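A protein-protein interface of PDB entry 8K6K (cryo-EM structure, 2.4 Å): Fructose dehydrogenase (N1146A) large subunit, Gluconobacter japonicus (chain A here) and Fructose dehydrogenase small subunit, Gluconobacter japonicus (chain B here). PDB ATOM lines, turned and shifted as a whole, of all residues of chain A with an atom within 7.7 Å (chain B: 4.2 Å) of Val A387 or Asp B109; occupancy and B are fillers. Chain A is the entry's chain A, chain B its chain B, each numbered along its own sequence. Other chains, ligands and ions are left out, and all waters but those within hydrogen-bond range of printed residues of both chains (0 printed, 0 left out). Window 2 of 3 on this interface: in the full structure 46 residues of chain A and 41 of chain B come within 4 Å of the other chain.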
ATOM      1  N   ALA A 381       4.004  24.985  29.993  1.00  0.00           N
ATOM      2  CA  ALA A 381       4.699  23.998  29.177  1.00  0.00           C
ATOM      3  C   ALA A 381       6.203  24.230  29.190  1.00  0.00           C
ATOM      4  O   ALA A 381       6.981  23.271  29.219  1.00  0.00           O
ATOM      5  CB  ALA A 381       4.161  24.024  27.750  1.00  0.00           C
ATOM      6  N   LEU A 382       6.633  25.493  29.163  1.00  0.00           N
ATOM      7  CA  LEU A 382       8.059  25.776  29.247  1.00  0.00           C
ATOM      8  C   LEU A 382       8.625  25.386  30.604  1.00  0.00           C
ATOM      9  O   LEU A 382       9.785  24.969  30.693  1.00  0.00           O
ATOM     10  CB  LEU A 382       8.320  27.254  28.965  1.00  0.00           C
ATOM     11  CG  LEU A 382       8.161  27.696  27.511  1.00  0.00           C
ATOM     12  CD1 LEU A 382       8.267  29.204  27.400  1.00  0.00           C
ATOM     13  CD2 LEU A 382       9.189  27.015  26.629  1.00  0.00           C
ATOM     14  N   MET A 384       7.779  22.826  32.218  1.00  0.00           N
ATOM     15  CA  MET A 384       7.807  21.372  32.275  1.00  0.00           C
ATOM     16  C   MET A 384       9.044  20.772  31.622  1.00  0.00           C
ATOM     17  O   MET A 384       9.192  19.547  31.621  1.00  0.00           O
ATOM     18  CB  MET A 384       6.554  20.791  31.615  1.00  0.00           C
ATOM     19  CG  MET A 384       5.288  20.957  32.431  1.00  0.00           C
ATOM     20  SD  MET A 384       3.807  20.887  31.414  1.00  0.00           S
ATOM     21  CE  MET A 384       3.563  19.118  31.309  1.00  0.00           C
ATOM     22  N   GLY A 385       9.926  21.596  31.067  1.00  0.00           N
ATOM     23  CA  GLY A 385      11.121  21.087  30.419  1.00  0.00           C
ATOM     24  C   GLY A 385      10.851  20.279  29.169  1.00  0.00           C
ATOM     25  O   GLY A 385      11.536  19.280  28.920  1.00  0.00           O
ATOM     26  N   LEU A 386       9.865  20.683  28.377  1.00  0.00           N
ATOM     27  CA  LEU A 386       9.538  19.991  27.143  1.00  0.00           C
ATOM     28  C   LEU A 386      10.303  20.603  25.976  1.00  0.00           C
ATOM     29  O   LEU A 386      10.809  21.724  26.050  1.00  0.00           O
ATOM     30  CB  LEU A 386       8.035  20.040  26.882  1.00  0.00           C
ATOM     31  CG  LEU A 386       7.221  19.130  27.798  1.00  0.00           C
ATOM     32  CD1 LEU A 386       5.778  19.566  27.825  1.00  0.00           C
ATOM     33  CD2 LEU A 386       7.336  17.683  27.359  1.00  0.00           C
ATOM     34  N   VAL A 387      10.380  19.845  24.886  1.00  0.00           N
ATOM     35  CA  VAL A 387      11.231  20.195  23.757  1.00  0.00           C
ATOM     36  C   VAL A 387      10.577  19.712  22.470  1.00  0.00           C
ATOM     37  O   VAL A 387       9.897  18.680  22.454  1.00  0.00           O
ATOM     38  CB  VAL A 387      12.646  19.598  23.935  1.00  0.00           C
ATOM     39  CG1 VAL A 387      12.998  18.639  22.806  1.00  0.00           C
ATOM     40  CG2 VAL A 387      13.674  20.701  24.048  1.00  0.00           C
ATOM     41  N   GLY A 388      10.761  20.477  21.397  1.00  0.00           N
ATOM     42  CA  GLY A 388      10.351  20.015  20.081  1.00  0.00           C
ATOM     43  C   GLY A 388       8.845  19.981  19.913  1.00  0.00           C
ATOM     44  O   GLY A 388       8.118  20.861  20.382  1.00  0.00           O
ATOM     45  N   LYS A 389       8.370  18.945  19.216  1.00  0.00           N
ATOM     46  CA  LYS A 389       6.943  18.821  18.941  1.00  0.00           C
ATOM     47  C   LYS A 389       6.137  18.608  20.213  1.00  0.00           C
ATOM     48  O   LYS A 389       4.972  19.013  20.279  1.00  0.00           O
ATOM     49  CB  LYS A 389       6.696  17.676  17.961  1.00  0.00           C
ATOM     50  CG  LYS A 389       7.014  18.022  16.521  1.00  0.00           C
ATOM     51  CD  LYS A 389       7.058  16.782  15.650  1.00  0.00           C
ATOM     52  CE  LYS A 389       7.144  17.149  14.179  1.00  0.00           C
ATOM     53  NZ  LYS A 389       7.593  18.555  13.987  1.00  0.00           N
ATOM     54  N   LYS A 390       6.729  17.968  21.223  1.00  0.00           N
ATOM     55  CA  LYS A 390       6.024  17.775  22.485  1.00  0.00           C
ATOM     56  C   LYS A 390       5.703  19.109  23.142  1.00  0.00           C
ATOM     57  O   LYS A 390       4.632  19.275  23.733  1.00  0.00           O
ATOM     58  CB  LYS A 390       6.852  16.899  23.421  1.00  0.00           C
ATOM     59  CG  LYS A 390       7.379  15.634  22.776  1.00  0.00           C
ATOM     60  CD  LYS A 390       6.625  14.414  23.267  1.00  0.00           C
ATOM     61  CE  LYS A 390       5.649  13.914  22.217  1.00  0.00           C
ATOM     62  NZ  LYS A 390       4.910  12.708  22.680  1.00  0.00           N
ATOM     63  N   LEU A 391       6.619  20.073  23.045  1.00  0.00           N
ATOM     64  CA  LEU A 391       6.374  21.392  23.619  1.00  0.00           C
ATOM     65  C   LEU A 391       5.186  22.073  22.949  1.00  0.00           C
ATOM     66  O   LEU A 391       4.307  22.620  23.625  1.00  0.00           O
ATOM     67  CB  LEU A 391       7.633  22.250  23.492  1.00  0.00           C
ATOM     68  CG  LEU A 391       7.551  23.704  23.951  1.00  0.00           C
ATOM     69  CD1 LEU A 391       7.166  23.783  25.412  1.00  0.00           C
ATOM     70  CD2 LEU A 391       8.874  24.398  23.712  1.00  0.00           C
ATOM     71  N   ASP A 392       5.140  22.044  21.615  1.00  0.00           N
ATOM     72  CA  ASP A 392       4.026  22.659  20.900  1.00  0.00           C
ATOM     73  C   ASP A 392       2.715  21.944  21.198  1.00  0.00           C
ATOM     74  O   ASP A 392       1.675  22.587  21.381  1.00  0.00           O
ATOM     75  CB  ASP A 392       4.303  22.660  19.399  1.00  0.00           C
ATOM     76  CG  ASP A 392       5.508  23.494  19.030  1.00  0.00           C
ATOM     77  OD1 ASP A 392       5.866  24.399  19.808  1.00  0.00           O
ATOM     78  OD2 ASP A 392       6.098  23.243  17.959  1.00  0.00           O
ATOM     79  N   GLU A 393       2.746  20.611  21.244  1.00  0.00           N
ATOM     80  CA  GLU A 393       1.539  19.856  21.555  1.00  0.00           C
ATOM     81  C   GLU A 393       1.032  20.188  22.950  1.00  0.00           C
ATOM     82  O   GLU A 393      -0.173  20.361  23.154  1.00  0.00           O
ATOM     83  CB  GLU A 393       1.804  18.358  21.423  1.00  0.00           C
ATOM     84  CG  GLU A 393       1.933  17.877  19.993  1.00  0.00           C
ATOM     85  CD  GLU A 393       2.404  16.441  19.903  1.00  0.00           C
ATOM     86  OE1 GLU A 393       2.529  15.789  20.961  1.00  0.00           O
ATOM     87  OE2 GLU A 393       2.649  15.963  18.777  1.00  0.00           O
ATOM     88  N   VAL B 105      15.772  18.388  17.757  1.00  0.00           N
ATOM     89  CA  VAL B 105      16.084  18.789  19.121  1.00  0.00           C
ATOM     90  C   VAL B 105      15.672  17.724  20.129  1.00  0.00           C
ATOM     91  O   VAL B 105      16.189  17.709  21.250  1.00  0.00           O
ATOM     92  CB  VAL B 105      15.422  20.142  19.440  1.00  0.00           C
ATOM     93  CG1 VAL B 105      13.919  19.991  19.531  1.00  0.00           C
ATOM     94  CG2 VAL B 105      15.990  20.734  20.720  1.00  0.00           C
ATOM     95  N   GLU B 106      14.761  16.822  19.761  1.00  0.00           N
ATOM     96  CA  GLU B 106      14.381  15.746  20.670  1.00  0.00           C
ATOM     97  C   GLU B 106      15.577  14.864  21.002  1.00  0.00           C
ATOM     98  O   GLU B 106      15.843  14.570  22.173  1.00  0.00           O
ATOM     99  CB  GLU B 106      13.255  14.911  20.060  1.00  0.00           C
ATOM    100  CG  GLU B 106      11.865  15.486  20.249  1.00  0.00           C
ATOM    101  CD  GLU B 106      11.508  16.517  19.198  1.00  0.00           C
ATOM    102  OE1 GLU B 106      12.393  16.894  18.403  1.00  0.00           O
ATOM    103  OE2 GLU B 106      10.336  16.944  19.164  1.00  0.00           O
ATOM    104  N   ALA B 107      16.318  14.438  19.975  1.00  0.00           N
ATOM    105  CA  ALA B 107      17.477  13.580  20.200  1.00  0.00           C
ATOM    106  C   ALA B 107      18.564  14.306  20.981  1.00  0.00           C
ATOM    107  O   ALA B 107      19.177  13.728  21.886  1.00  0.00           O
ATOM    108  CB  ALA B 107      18.021  13.074  18.865  1.00  0.00           C
ATOM    109  N   LEU B 108      18.820  15.570  20.640  1.00  0.00           N
ATOM    110  CA  LEU B 108      19.840  16.335  21.349  1.00  0.00           C
ATOM    111  C   LEU B 108      19.476  16.509  22.817  1.00  0.00           C
ATOM    112  O   LEU B 108      20.332  16.369  23.697  1.00  0.00           O
ATOM    113  CB  LEU B 108      20.038  17.692  20.675  1.00  0.00           C
ATOM    114  CG  LEU B 108      20.803  18.751  21.465  1.00  0.00           C
ATOM    115  CD1 LEU B 108      22.296  18.517  21.356  1.00  0.00           C
ATOM    116  CD2 LEU B 108      20.447  20.139  20.973  1.00  0.00           C
ATOM    117  N   ASP B 109      18.209  16.813  23.100  1.00  0.00           N
ATOM    118  CA  ASP B 109      17.768  16.953  24.483  1.00  0.00           C
ATOM    119  C   ASP B 109      17.851  15.629  25.230  1.00  0.00           C
ATOM    120  O   ASP B 109      18.251  15.595  26.399  1.00  0.00           O
ATOM    121  CB  ASP B 109      16.344  17.503  24.522  1.00  0.00           C
ATOM    122  CG  ASP B 109      15.879  17.816  25.926  1.00  0.00           C
ATOM    123  OD1 ASP B 109      16.318  18.842  26.482  1.00  0.00           O
ATOM    124  OD2 ASP B 109      15.074  17.035  26.475  1.00  0.00           O
ATOM    125  N   ALA B 110      17.472  14.528  24.577  1.00  0.00           N
ATOM    126  CA  ALA B 110      17.523  13.227  25.235  1.00  0.00           C
ATOM    127  C   ALA B 110      18.955  12.815  25.545  1.00  0.00           C
ATOM    128  O   ALA B 110      19.224  12.235  26.603  1.00  0.00           O
ATOM    129  CB  ALA B 110      16.838  12.174  24.365  1.00  0.00           C
ATOM    130  N   ALA B 111      19.886  13.103  24.641  1.00  0.00           N
ATOM    131  CA  ALA B 111      21.272  12.685  24.800  1.00  0.00           C
ATOM    132  C   ALA B 111      22.120  13.686  25.572  1.00  0.00           C
ATOM    133  O   ALA B 111      23.303  13.421  25.803  1.00  0.00           O
ATOM    134  CB  ALA B 111      21.902  12.429  23.428  1.00  0.00           C
ATOM    135  N   MET B 112      21.553  14.820  25.978  1.00  0.00           N
ATOM    136  CA  MET B 112      22.289  15.831  26.730  1.00  0.00           C
ATOM    137  C   MET B 112      21.558  16.202  28.014  1.00  0.00           C
ATOM    138  O   MET B 112      21.557  17.366  28.418  1.00  0.00           O
ATOM    139  CB  MET B 112      22.532  17.076  25.879  1.00  0.00           C
ATOM    140  CG  MET B 112      23.884  17.110  25.192  1.00  0.00           C
ATOM    141  SD  MET B 112      24.248  18.711  24.448  1.00  0.00           S
ATOM    142  CE  MET B 112      23.009  19.743  25.225  1.00  0.00           C
ATOM    143  N   LYS B 113      20.927  15.222  28.664  1.00  0.00           N
ATOM    144  CA  LYS B 113      20.159  15.510  29.870  1.00  0.00           C
ATOM    145  C   LYS B 113      21.050  15.976  31.014  1.00  0.00           C
ATOM    146  O   LYS B 113      20.669  16.883  31.762  1.00  0.00           O
ATOM    147  CB  LYS B 113      19.359  14.277  30.288  1.00  0.00           C
ATOM    148  CG  LYS B 113      18.203  13.951  29.358  1.00  0.00           C
ATOM    149  CD  LYS B 113      16.933  13.644  30.130  1.00  0.00           C
ATOM    150  CE  LYS B 113      15.701  13.859  29.264  1.00  0.00           C
ATOM    151  NZ  LYS B 113      14.439  13.681  30.033  1.00  0.00           N
ATOM    152  N   HIS B 118      23.011  21.703  28.640  1.00  0.00           N
ATOM    153  CA  HIS B 118      21.552  21.627  28.654  1.00  0.00           C
ATOM    154  C   HIS B 118      20.890  22.903  29.159  1.00  0.00           C
ATOM    155  O   HIS B 118      19.908  23.346  28.537  1.00  0.00           O
ATOM    156  CB  HIS B 118      21.110  20.414  29.477  1.00  0.00           C
ATOM    157  CG  HIS B 118      19.777  19.866  29.081  1.00  0.00           C
ATOM    158  ND1 HIS B 118      18.766  19.645  29.991  1.00  0.00           N
ATOM    159  CD2 HIS B 118      19.287  19.490  27.877  1.00  0.00           C
ATOM    160  CE1 HIS B 118      17.710  19.159  29.364  1.00  0.00           C
ATOM    161  NE2 HIS B 118      18.001  19.055  28.080  1.00  0.00           N
ATOM    162  N   ILE B 122      18.057  24.995  26.952  1.00  0.00           N
ATOM    163  CA  ILE B 122      16.719  25.230  27.487  1.00  0.00           C
ATOM    164  C   ILE B 122      16.448  26.724  27.605  1.00  0.00           C
ATOM    165  O   ILE B 122      15.330  27.187  27.360  1.00  0.00           O
ATOM    166  CB  ILE B 122      16.549  24.507  28.835  1.00  0.00           C
ATOM    167  CG1 ILE B 122      16.671  22.997  28.640  1.00  0.00           C
ATOM    168  CG2 ILE B 122      15.212  24.848  29.464  1.00  0.00           C
ATOM    169  CD1 ILE B 122      15.582  22.406  27.780  1.00  0.00           C
ATOM    170  N   ILE B 125      15.604  28.014  24.129  1.00  0.00           N
ATOM    171  CA  ILE B 125      14.244  27.628  23.761  1.00  0.00           C
ATOM    172  C   ILE B 125      13.225  28.478  24.510  1.00  0.00           C
ATOM    173  O   ILE B 125      12.234  28.940  23.932  1.00  0.00           O
ATOM    174  CB  ILE B 125      14.032  26.127  24.018  1.00  0.00           C
ATOM    175  CG1 ILE B 125      14.912  25.309  23.076  1.00  0.00           C
ATOM    176  CG2 ILE B 125      12.575  25.754  23.841  1.00  0.00           C
ATOM    177  CD1 ILE B 125      15.123  23.897  23.528  1.00  0.00           C
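Among the printed residues, pairs that only touch across the chains: Gly A388 with Glu B106 (3.2 Å), Val A387 with Ile B125 (3.5 Å), Gly A388 with Val B105 (3.6 Å), Val A387 with Val B105 (3.7 Å), Val A387 with Glu B106 (3.7 Å), Val A387 with Asp B109 (3.9 Å) and Leu A391 with Ile B125 (3.9 Å).
Of the 12 printed residues of chain B, 4 touch a printed residue of chain A.
Printed residues of chain B that touch a printed residue of chain A: Val B105, Glu B106, Asp B109 and Ile B125.
Hydrophobic or aromatic side chains of chain B within 4 Å of the printed part of chain A: Val B105 and Ile B125.
Hydrophobic or aromatic side chains of chain A that line the printed part of chain B: Val A387 and Leu A391.
N of Lys A389 sits at hydrogen-bond distance from OE2 of Glu B106 (2.8 Å).
Of chain B, only Val B105, Glu B106, Asp B109 and Ile B125 come within 4 Å of Val A387.
Asp B109 touches just one residue of chain A: Val A387.
Of the printed residues of chain A, Glu B106 touches Val A387 (3.7 Å), Gly A388 (3.2 Å) and Lys A389 (2.8 Å).
Of the printed residues of chain A, Val B105 touches Val A387 and Gly A388.
Of the printed residues of chain A, Ile B125 touches Val A387 (3.5 Å) and Leu A391 (3.9 Å).
His B118 touches none of the printed residues of chain A.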
